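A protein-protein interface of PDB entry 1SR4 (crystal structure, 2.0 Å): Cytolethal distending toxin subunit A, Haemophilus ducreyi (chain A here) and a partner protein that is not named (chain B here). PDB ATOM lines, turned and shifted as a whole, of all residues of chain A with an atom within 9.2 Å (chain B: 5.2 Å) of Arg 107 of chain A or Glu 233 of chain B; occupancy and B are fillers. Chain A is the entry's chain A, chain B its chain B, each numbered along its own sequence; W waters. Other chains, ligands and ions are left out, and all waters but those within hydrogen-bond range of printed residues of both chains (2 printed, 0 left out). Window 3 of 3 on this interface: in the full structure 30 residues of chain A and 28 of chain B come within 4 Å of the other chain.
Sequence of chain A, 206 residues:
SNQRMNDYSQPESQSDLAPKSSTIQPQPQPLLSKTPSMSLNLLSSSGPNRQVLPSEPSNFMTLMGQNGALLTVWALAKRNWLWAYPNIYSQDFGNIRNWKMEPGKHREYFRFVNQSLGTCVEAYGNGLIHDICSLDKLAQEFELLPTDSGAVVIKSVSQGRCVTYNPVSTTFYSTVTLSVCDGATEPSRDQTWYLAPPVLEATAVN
The side-chain carboxylate (OE1) of Glu 233 of chain B sits close to the side-chain carboxylate (OD2) of Asp 222 of chain B, 2.6 Å away. NE of Arg 234 of chain B is in salt-bridge range of OD2 of Asp 260 of chain B, 3.0 Å away.
Of the 14 printed residues of chain A, 2 touch a printed residue of chain B. Printed residues of chain A that touch a printed residue of chain B: Arg 107 and Glu 108. Of the 16 printed residues of chain B, 6 touch a printed residue of chain A. Along chain B the printed residues that touch a printed residue of chain A span positions 233 to 260.
Arg 234 of chain B touches Arg 107 of chain A (CA to NH2, 3.9 Å). Gly 236 of chain B touches Arg 107 of chain A. Ala 237 of chain B touches Glu 108 of chain A (O to CG, 3.4 Å).
Water W1 lies within hydrogen-bond range of the backbone NH (N) of Glu 108 of chain A and the backbone carbonyl oxygen (O) of Ala 237 of chain B. Water W2 lies within hydrogen-bond range of O of Ile 235 of chain B (3.0 Å), O of Glu 233 of chain B (3.0 Å) and NH1 of Arg 107 of chain A (3.1 Å).
Printed residues of chain B within 4 Å of Glu 108 of chain A: Ala 237 (3.4 Å). Phe 110 of chain A touches none of the printed residues of chain B. Of chain A, only Arg 107 comes within 4 Å of Glu 233 of chain B. Printed residues of chain A within 4 Å of Ala 237 of chain B: Glu 108. The nearest residue of chain B that does not touch Arg 107 of chain A is Ala 237 of chain B (4.8 Å). The nearest printed residue of chain A that does not touch Glu 233 of chain B is Lys 105 of chain A (11.1 Å).
O of Ile 235 of chain B is in hydrogen-bond range of NH2 of Arg 107 of chain A. NH2 of Arg 107 of chain A is in hydrogen-bond range of O of Glu 233 of chain B (3.2 Å). OD2 of Asp 260 of chain B is in salt-bridge range of NH2 of Arg 107 of chain A (2.8 Å).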
ATOM      1  N   PRO A 103     -15.726   5.046  -6.313  1.00  0.00           N
ATOM      2  CA  PRO A 103     -16.259   3.790  -6.819  1.00  0.00           C
ATOM      3  C   PRO A 103     -17.228   4.166  -7.925  1.00  0.00           C
ATOM      4  O   PRO A 103     -17.818   5.242  -7.895  1.00  0.00           O
ATOM      5  CB  PRO A 103     -16.965   3.199  -5.597  1.00  0.00           C
ATOM      6  CG  PRO A 103     -16.072   3.631  -4.482  1.00  0.00           C
ATOM      7  CD  PRO A 103     -15.832   5.094  -4.840  1.00  0.00           C
ATOM      8  N   GLY A 104     -17.381   3.298  -8.910  1.00  0.00           N
ATOM      9  CA  GLY A 104     -18.301   3.599  -9.984  1.00  0.00           C
ATOM     10  C   GLY A 104     -19.672   3.041  -9.670  1.00  0.00           C
ATOM     11  O   GLY A 104     -19.944   2.614  -8.551  1.00  0.00           O
ATOM     12  N   LYS A 105     -20.535   3.045 -10.668  1.00  0.00           N
ATOM     13  CA  LYS A 105     -21.879   2.525 -10.528  1.00  0.00           C
ATOM     14  C   LYS A 105     -21.807   1.029 -10.253  1.00  0.00           C
ATOM     15  O   LYS A 105     -22.537   0.514  -9.405  1.00  0.00           O
ATOM     16  CB  LYS A 105     -22.651   2.780 -11.821  1.00  0.00           C
ATOM     17  CG  LYS A 105     -24.045   2.168 -11.893  1.00  0.00           C
ATOM     18  CD  LYS A 105     -24.546   2.257 -13.336  1.00  0.00           C
ATOM     19  CE  LYS A 105     -26.034   1.981 -13.463  1.00  0.00           C
ATOM     20  NZ  LYS A 105     -26.490   2.186 -14.876  1.00  0.00           N
ATOM     21  N   HIS A 106     -20.929   0.332 -10.971  1.00  0.00           N
ATOM     22  CA  HIS A 106     -20.791  -1.112 -10.799  1.00  0.00           C
ATOM     23  C   HIS A 106     -19.781  -1.501  -9.728  1.00  0.00           C
ATOM     24  O   HIS A 106     -18.805  -0.797  -9.495  1.00  0.00           O
ATOM     25  CB  HIS A 106     -20.390  -1.759 -12.125  1.00  0.00           C
ATOM     26  CG  HIS A 106     -21.406  -1.587 -13.205  1.00  0.00           C
ATOM     27  ND1 HIS A 106     -21.679  -0.366 -13.784  1.00  0.00           N
ATOM     28  CD2 HIS A 106     -22.228  -2.479 -13.806  1.00  0.00           C
ATOM     29  CE1 HIS A 106     -22.624  -0.514 -14.695  1.00  0.00           C
ATOM     30  NE2 HIS A 106     -22.974  -1.787 -14.728  1.00  0.00           N
ATOM     31  N   ARG A 107     -20.003  -2.637  -9.082  1.00  0.00           N
ATOM     32  CA  ARG A 107     -19.080  -3.073  -8.038  1.00  0.00           C
ATOM     33  C   ARG A 107     -17.692  -3.338  -8.608  1.00  0.00           C
ATOM     34  O   ARG A 107     -17.548  -3.830  -9.727  1.00  0.00           O
ATOM     35  CB  ARG A 107     -19.609  -4.335  -7.344  1.00  0.00           C
ATOM     36  CG  ARG A 107     -20.874  -4.070  -6.539  1.00  0.00           C
ATOM     37  CD  ARG A 107     -21.419  -5.319  -5.863  1.00  0.00           C
ATOM     38  NE  ARG A 107     -22.649  -5.009  -5.144  1.00  0.00           N
ATOM     39  CZ  ARG A 107     -23.331  -5.880  -4.411  1.00  0.00           C
ATOM     40  NH1 ARG A 107     -22.902  -7.132  -4.294  1.00  0.00           N
ATOM     41  NH2 ARG A 107     -24.436  -5.496  -3.789  1.00  0.00           N
ATOM     42  N   GLU A 108     -16.681  -2.983  -7.828  1.00  0.00           N
ATOM     43  CA  GLU A 108     -15.279  -3.186  -8.191  1.00  0.00           C
ATOM     44  C   GLU A 108     -14.699  -2.237  -9.235  1.00  0.00           C
ATOM     45  O   GLU A 108     -13.520  -2.339  -9.569  1.00  0.00           O
ATOM     46  CB  GLU A 108     -15.049  -4.643  -8.606  1.00  0.00           C
ATOM     47  CG  GLU A 108     -15.316  -5.628  -7.465  1.00  0.00           C
ATOM     48  CD  GLU A 108     -14.786  -7.021  -7.762  1.00  0.00           C
ATOM     49  OE1 GLU A 108     -15.475  -7.771  -8.488  1.00  0.00           O
ATOM     50  OE2 GLU A 108     -13.675  -7.355  -7.286  1.00  0.00           O
ATOM     51  N   TYR A 109     -15.506  -1.313  -9.755  1.00  0.00           N
ATOM     52  CA  TYR A 109     -14.977  -0.356 -10.721  1.00  0.00           C
ATOM     53  C   TYR A 109     -14.808   1.029 -10.102  1.00  0.00           C
ATOM     54  O   TYR A 109     -15.439   1.369  -9.084  1.00  0.00           O
ATOM     55  CB  TYR A 109     -15.874  -0.233 -11.953  1.00  0.00           C
ATOM     56  CG  TYR A 109     -16.151  -1.534 -12.681  1.00  0.00           C
ATOM     57  CD1 TYR A 109     -15.262  -2.607 -12.617  1.00  0.00           C
ATOM     58  CD2 TYR A 109     -17.298  -1.673 -13.457  1.00  0.00           C
ATOM     59  CE1 TYR A 109     -15.514  -3.789 -13.311  1.00  0.00           C
ATOM     60  CE2 TYR A 109     -17.558  -2.842 -14.157  1.00  0.00           C
ATOM     61  CZ  TYR A 109     -16.663  -3.896 -14.079  1.00  0.00           C
ATOM     62  OH  TYR A 109     -16.923  -5.042 -14.792  1.00  0.00           O
ATOM     63  N   PHE A 110     -13.956   1.829 -10.733  1.00  0.00           N
ATOM     64  CA  PHE A 110     -13.679   3.177 -10.273  1.00  0.00           C
ATOM     65  C   PHE A 110     -13.777   4.179 -11.405  1.00  0.00           C
ATOM     66  O   PHE A 110     -13.657   3.831 -12.591  1.00  0.00           O
ATOM     67  CB  PHE A 110     -12.270   3.240  -9.684  1.00  0.00           C
ATOM     68  CG  PHE A 110     -12.104   2.414  -8.448  1.00  0.00           C
ATOM     69  CD1 PHE A 110     -12.548   2.890  -7.218  1.00  0.00           C
ATOM     70  CD2 PHE A 110     -11.537   1.137  -8.518  1.00  0.00           C
ATOM     71  CE1 PHE A 110     -12.434   2.114  -6.060  1.00  0.00           C
ATOM     72  CE2 PHE A 110     -11.418   0.350  -7.367  1.00  0.00           C
ATOM     73  CZ  PHE A 110     -11.871   0.847  -6.134  1.00  0.00           C
ATOM     74  N   LEU A 138     -20.568   3.606 -18.926  1.00  0.00           N
ATOM     75  CA  LEU A 138     -19.609   2.538 -18.675  1.00  0.00           C
ATOM     76  C   LEU A 138     -18.191   2.942 -19.096  1.00  0.00           C
ATOM     77  O   LEU A 138     -17.210   2.519 -18.478  1.00  0.00           O
ATOM     78  CB  LEU A 138     -20.031   1.266 -19.424  1.00  0.00           C
ATOM     79  CG  LEU A 138     -19.396  -0.043 -18.948  1.00  0.00           C
ATOM     80  CD1 LEU A 138     -19.793  -0.287 -17.485  1.00  0.00           C
ATOM     81  CD2 LEU A 138     -19.860  -1.214 -19.828  1.00  0.00           C
ATOM     82  N   GLU A 141     -15.895   4.056 -16.419  1.00  0.00           N
ATOM     83  CA  GLU A 141     -15.614   3.108 -15.350  1.00  0.00           C
ATOM     84  C   GLU A 141     -14.390   2.282 -15.694  1.00  0.00           C
ATOM     85  O   GLU A 141     -14.238   1.825 -16.831  1.00  0.00           O
ATOM     86  CB  GLU A 141     -16.811   2.184 -15.122  1.00  0.00           C
ATOM     87  CG  GLU A 141     -18.021   2.862 -14.475  1.00  0.00           C
ATOM     88  CD  GLU A 141     -18.999   1.846 -13.904  1.00  0.00           C
ATOM     89  OE1 GLU A 141     -18.821   1.416 -12.747  1.00  0.00           O
ATOM     90  OE2 GLU A 141     -19.935   1.454 -14.628  1.00  0.00           O
ATOM     91  N   PHE A 142     -13.516   2.093 -14.707  1.00  0.00           N
ATOM     92  CA  PHE A 142     -12.280   1.351 -14.898  1.00  0.00           C
ATOM     93  C   PHE A 142     -12.045   0.310 -13.808  1.00  0.00           C
ATOM     94  O   PHE A 142     -12.411   0.499 -12.649  1.00  0.00           O
ATOM     95  CB  PHE A 142     -11.083   2.321 -14.922  1.00  0.00           C
ATOM     96  CG  PHE A 142     -11.124   3.310 -16.055  1.00  0.00           C
ATOM     97  CD1 PHE A 142     -10.483   3.034 -17.261  1.00  0.00           C
ATOM     98  CD2 PHE A 142     -11.842   4.491 -15.937  1.00  0.00           C
ATOM     99  CE1 PHE A 142     -10.554   3.918 -18.332  1.00  0.00           C
ATOM    100  CE2 PHE A 142     -11.923   5.381 -17.007  1.00  0.00           C
ATOM    101  CZ  PHE A 142     -11.272   5.088 -18.214  1.00  0.00           C
ATOM    102  N   GLU A 143     -11.454  -0.808 -14.202  1.00  0.00           N
ATOM    103  CA  GLU A 143     -11.112  -1.859 -13.259  1.00  0.00           C
ATOM    104  C   GLU A 143      -9.601  -1.764 -13.085  1.00  0.00           C
ATOM    105  O   GLU A 143      -8.862  -1.785 -14.065  1.00  0.00           O
ATOM    106  CB  GLU A 143     -11.473  -3.250 -13.809  1.00  0.00           C
ATOM    107  CG  GLU A 143     -10.977  -4.379 -12.890  1.00  0.00           C
ATOM    108  CD  GLU A 143     -11.509  -5.774 -13.240  1.00  0.00           C
ATOM    109  OE1 GLU A 143     -11.400  -6.200 -14.414  1.00  0.00           O
ATOM    110  OE2 GLU A 143     -12.018  -6.452 -12.316  1.00  0.00           O
ATOM    111  N   LEU A 144      -9.126  -1.629 -11.857  1.00  0.00           N
ATOM    112  CA  LEU A 144      -7.682  -1.576 -11.651  1.00  0.00           C
ATOM    113  C   LEU A 144      -7.261  -2.956 -11.186  1.00  0.00           C
ATOM    114  O   LEU A 144      -7.784  -3.479 -10.204  1.00  0.00           O
ATOM    115  CB  LEU A 144      -7.305  -0.508 -10.618  1.00  0.00           C
ATOM    116  CG  LEU A 144      -7.197   0.921 -11.169  1.00  0.00           C
ATOM    117  CD1 LEU A 144      -8.518   1.334 -11.810  1.00  0.00           C
ATOM    118  CD2 LEU A 144      -6.811   1.878 -10.045  1.00  0.00           C
ATOM    119  N   VAL A 157     -13.407  -0.693 -18.763  1.00  0.00           N
ATOM    120  CA  VAL A 157     -14.425  -1.735 -18.731  1.00  0.00           C
ATOM    121  C   VAL A 157     -15.232  -1.754 -20.031  1.00  0.00           C
ATOM    122  O   VAL A 157     -15.578  -2.822 -20.541  1.00  0.00           O
ATOM    123  CB  VAL A 157     -15.375  -1.550 -17.541  1.00  0.00           C
ATOM    124  CG1 VAL A 157     -16.516  -2.562 -17.625  1.00  0.00           C
ATOM    125  CG2 VAL A 157     -14.595  -1.725 -16.229  1.00  0.00           C
ATOM    126  N   SER B   3     -24.998  -1.082   6.029  1.00  0.00           N
ATOM    127  CA  SER B   3     -24.693  -0.322   4.822  1.00  0.00           C
ATOM    128  C   SER B   3     -24.432   1.166   5.064  1.00  0.00           C
ATOM    129  O   SER B   3     -23.959   1.859   4.163  1.00  0.00           O
ATOM    130  CB  SER B   3     -25.800  -0.502   3.768  1.00  0.00           C
ATOM    131  OG  SER B   3     -26.998   0.164   4.136  1.00  0.00           O
ATOM    132  N   ILE B 200     -24.599 -13.901   3.938  1.00  0.00           N
ATOM    133  CA  ILE B 200     -24.223 -13.696   2.557  1.00  0.00           C
ATOM    134  C   ILE B 200     -22.749 -13.305   2.531  1.00  0.00           C
ATOM    135  O   ILE B 200     -22.318 -12.438   3.290  1.00  0.00           O
ATOM    136  CB  ILE B 200     -25.132 -12.610   1.898  1.00  0.00           C
ATOM    137  CG1 ILE B 200     -24.941 -12.600   0.377  1.00  0.00           C
ATOM    138  CG2 ILE B 200     -24.900 -11.257   2.559  1.00  0.00           C
ATOM    139  CD1 ILE B 200     -23.771 -11.866  -0.091  1.00  0.00           C
ATOM    140  N   ILE B 202     -19.676 -11.513   0.920  1.00  0.00           N
ATOM    141  CA  ILE B 202     -19.433 -10.376   0.032  1.00  0.00           C
ATOM    142  C   ILE B 202     -17.923 -10.328  -0.182  1.00  0.00           C
ATOM    143  O   ILE B 202     -17.161 -10.084   0.769  1.00  0.00           O
ATOM    144  CB  ILE B 202     -19.912  -9.021   0.651  1.00  0.00           C
ATOM    145  CG1 ILE B 202     -21.444  -8.991   0.776  1.00  0.00           C
ATOM    146  CG2 ILE B 202     -19.556  -7.870  -0.274  1.00  0.00           C
ATOM    147  CD1 ILE B 202     -21.975  -9.735   1.951  1.00  0.00           C
ATOM    148  N   LEU B 220     -21.849 -11.540   6.095  1.00  0.00           N
ATOM    149  CA  LEU B 220     -22.709 -10.778   6.993  1.00  0.00           C
ATOM    150  C   LEU B 220     -24.126 -11.279   7.148  1.00  0.00           C
ATOM    151  O   LEU B 220     -24.604 -12.083   6.360  1.00  0.00           O
ATOM    152  CB  LEU B 220     -22.751  -9.321   6.541  1.00  0.00           C
ATOM    153  CG  LEU B 220     -23.328  -9.005   5.165  1.00  0.00           C
ATOM    154  CD1 LEU B 220     -24.851  -8.907   5.241  1.00  0.00           C
ATOM    155  CD2 LEU B 220     -22.763  -7.665   4.691  1.00  0.00           C
ATOM    156  N   ASP B 222     -27.791  -9.492   7.709  1.00  0.00           N
ATOM    157  CA  ASP B 222     -28.526  -8.236   7.795  1.00  0.00           C
ATOM    158  C   ASP B 222     -29.879  -8.540   8.426  1.00  0.00           C
ATOM    159  O   ASP B 222     -30.727  -9.162   7.796  1.00  0.00           O
ATOM    160  CB  ASP B 222     -28.748  -7.635   6.412  1.00  0.00           C
ATOM    161  CG  ASP B 222     -29.484  -6.308   6.472  1.00  0.00           C
ATOM    162  OD1 ASP B 222     -30.163  -6.030   7.484  1.00  0.00           O
ATOM    163  OD2 ASP B 222     -29.395  -5.540   5.500  1.00  0.00           O
ATOM    164  N   LEU B 225     -33.178  -8.312   6.561  1.00  0.00           N
ATOM    165  CA  LEU B 225     -33.555  -9.211   5.486  1.00  0.00           C
ATOM    166  C   LEU B 225     -33.932 -10.592   6.007  1.00  0.00           C
ATOM    167  O   LEU B 225     -33.338 -11.093   6.957  1.00  0.00           O
ATOM    168  CB  LEU B 225     -32.417  -9.297   4.461  1.00  0.00           C
ATOM    169  CG  LEU B 225     -31.986  -7.982   3.776  1.00  0.00           C
ATOM    170  CD1 LEU B 225     -30.809  -8.253   2.837  1.00  0.00           C
ATOM    171  CD2 LEU B 225     -33.155  -7.379   2.988  1.00  0.00           C
ATOM    172  N   GLU B 229     -32.901 -14.477   1.830  1.00  0.00           N
ATOM    173  CA  GLU B 229     -32.998 -13.229   1.072  1.00  0.00           C
ATOM    174  C   GLU B 229     -31.824 -12.269   1.308  1.00  0.00           C
ATOM    175  O   GLU B 229     -31.878 -11.104   0.905  1.00  0.00           O
ATOM    176  CB  GLU B 229     -34.307 -12.524   1.431  1.00  0.00           C
ATOM    177  CG  GLU B 229     -35.539 -13.407   1.283  1.00  0.00           C
ATOM    178  CD  GLU B 229     -36.157 -13.327  -0.098  1.00  0.00           C
ATOM    179  OE1 GLU B 229     -35.429 -12.967  -1.045  1.00  0.00           O
ATOM    180  OE2 GLU B 229     -37.368 -13.630  -0.237  1.00  0.00           O
ATOM    181  N   GLN B 230     -30.765 -12.752   1.952  1.00  0.00           N
ATOM    182  CA  GLN B 230     -29.603 -11.906   2.243  1.00  0.00           C
ATOM    183  C   GLN B 230     -28.914 -11.358   0.979  1.00  0.00           C
ATOM    184  O   GLN B 230     -28.263 -10.306   1.014  1.00  0.00           O
ATOM    185  CB  GLN B 230     -28.609 -12.695   3.087  1.00  0.00           C
ATOM    186  CG  GLN B 230     -29.162 -13.134   4.451  1.00  0.00           C
ATOM    187  CD  GLN B 230     -29.306 -11.976   5.408  1.00  0.00           C
ATOM    188  OE1 GLN B 230     -28.419 -11.136   5.507  1.00  0.00           O
ATOM    189  NE2 GLN B 230     -30.423 -11.920   6.116  1.00  0.00           N
ATOM    190  N   ALA B 231     -29.073 -12.051  -0.144  1.00  0.00           N
ATOM    191  CA  ALA B 231     -28.451 -11.598  -1.382  1.00  0.00           C
ATOM    192  C   ALA B 231     -29.036 -10.257  -1.848  1.00  0.00           C
ATOM    193  O   ALA B 231     -28.570  -9.680  -2.822  1.00  0.00           O
ATOM    194  CB  ALA B 231     -28.598 -12.659  -2.467  1.00  0.00           C
ATOM    195  N   ARG B 232     -30.058  -9.760  -1.155  1.00  0.00           N
ATOM    196  CA  ARG B 232     -30.627  -8.462  -1.510  1.00  0.00           C
ATOM    197  C   ARG B 232     -29.744  -7.337  -0.939  1.00  0.00           C
ATOM    198  O   ARG B 232     -29.983  -6.159  -1.195  1.00  0.00           O
ATOM    199  CB  ARG B 232     -32.049  -8.314  -0.955  1.00  0.00           C
ATOM    200  CG  ARG B 232     -33.139  -9.097  -1.706  1.00  0.00           C
ATOM    201  CD  ARG B 232     -34.488  -8.858  -1.024  1.00  0.00           C
ATOM    202  NE  ARG B 232     -35.605  -9.575  -1.639  1.00  0.00           N
ATOM    203  CZ  ARG B 232     -36.103  -9.323  -2.851  1.00  0.00           C
ATOM    204  NH1 ARG B 232     -37.127 -10.040  -3.309  1.00  0.00           N
ATOM    205  NH2 ARG B 232     -35.585  -8.358  -3.608  1.00  0.00           N
ATOM    206  N   GLU B 233     -28.723  -7.700  -0.165  1.00  0.00           N
ATOM    207  CA  GLU B 233     -27.836  -6.698   0.432  1.00  0.00           C
ATOM    208  C   GLU B 233     -27.193  -5.757  -0.605  1.00  0.00           C
ATOM    209  O   GLU B 233     -26.640  -6.202  -1.601  1.00  0.00           O
ATOM    210  CB  GLU B 233     -26.727  -7.390   1.231  1.00  0.00           C
ATOM    211  CG  GLU B 233     -25.950  -6.442   2.151  1.00  0.00           C
ATOM    212  CD  GLU B 233     -26.839  -5.794   3.199  1.00  0.00           C
ATOM    213  OE1 GLU B 233     -27.625  -6.525   3.833  1.00  0.00           O
ATOM    214  OE2 GLU B 233     -26.754  -4.559   3.398  1.00  0.00           O
ATOM    215  N   ARG B 234     -27.249  -4.455  -0.356  1.00  0.00           N
ATOM    216  CA  ARG B 234     -26.661  -3.501  -1.286  1.00  0.00           C
ATOM    217  C   ARG B 234     -25.266  -3.067  -0.841  1.00  0.00           C
ATOM    218  O   ARG B 234     -24.931  -1.886  -0.859  1.00  0.00           O
ATOM    219  CB  ARG B 234     -27.570  -2.276  -1.441  1.00  0.00           C
ATOM    220  CG  ARG B 234     -28.949  -2.627  -1.990  1.00  0.00           C
ATOM    221  CD  ARG B 234     -28.820  -3.372  -3.305  1.00  0.00           C
ATOM    222  NE  ARG B 234     -28.168  -2.542  -4.318  1.00  0.00           N
ATOM    223  CZ  ARG B 234     -28.789  -1.598  -5.020  1.00  0.00           C
ATOM    224  NH1 ARG B 234     -30.087  -1.370  -4.827  1.00  0.00           N
ATOM    225  NH2 ARG B 234     -28.113  -0.863  -5.895  1.00  0.00           N
ATOM    226  N   ILE B 235     -24.463  -4.037  -0.417  1.00  0.00           N
ATOM    227  CA  ILE B 235     -23.095  -3.760   0.008  1.00  0.00           C
ATOM    228  C   ILE B 235     -22.172  -4.513  -0.940  1.00  0.00           C
ATOM    229  O   ILE B 235     -22.338  -5.706  -1.145  1.00  0.00           O
ATOM    230  CB  ILE B 235     -22.855  -4.222   1.453  1.00  0.00           C
ATOM    231  CG1 ILE B 235     -23.755  -3.421   2.401  1.00  0.00           C
ATOM    232  CG2 ILE B 235     -21.370  -4.050   1.825  1.00  0.00           C
ATOM    233  CD1 ILE B 235     -23.576  -3.767   3.901  1.00  0.00           C
ATOM    234  N   GLY B 236     -21.220  -3.808  -1.549  1.00  0.00           N
ATOM    235  CA  GLY B 236     -20.305  -4.466  -2.466  1.00  0.00           C
ATOM    236  C   GLY B 236     -18.872  -4.457  -1.950  1.00  0.00           C
ATOM    237  O   GLY B 236     -18.457  -3.505  -1.269  1.00  0.00           O
ATOM    238  N   ALA B 237     -18.112  -5.505  -2.269  1.00  0.00           N
ATOM    239  CA  ALA B 237     -16.711  -5.585  -1.849  1.00  0.00           C
ATOM    240  C   ALA B 237     -15.838  -5.081  -2.988  1.00  0.00           C
ATOM    241  O   ALA B 237     -16.172  -5.258  -4.153  1.00  0.00           O
ATOM    242  CB  ALA B 237     -16.337  -7.022  -1.510  1.00  0.00           C
ATOM    243  N   ASP B 260     -23.805   0.216  -2.408  1.00  0.00           N
ATOM    244  CA  ASP B 260     -23.786   0.472  -3.846  1.00  0.00           C
ATOM    245  C   ASP B 260     -24.309   1.891  -4.074  1.00  0.00           C
ATOM    246  O   ASP B 260     -25.227   2.341  -3.387  1.00  0.00           O
ATOM    247  CB  ASP B 260     -24.695  -0.498  -4.617  1.00  0.00           C
ATOM    248  CG  ASP B 260     -24.274  -1.951  -4.470  1.00  0.00           C
ATOM    249  OD1 ASP B 260     -23.063  -2.229  -4.485  1.00  0.00           O
ATOM    250  OD2 ASP B 260     -25.161  -2.824  -4.360  1.00  0.00           O
HETATM  251  O   HOH W   1     -17.912  -2.879  -5.208  1.00  0.00           O
HETATM  252  O   HOH W   2     -24.175  -7.976  -1.590  1.00  0.00           O
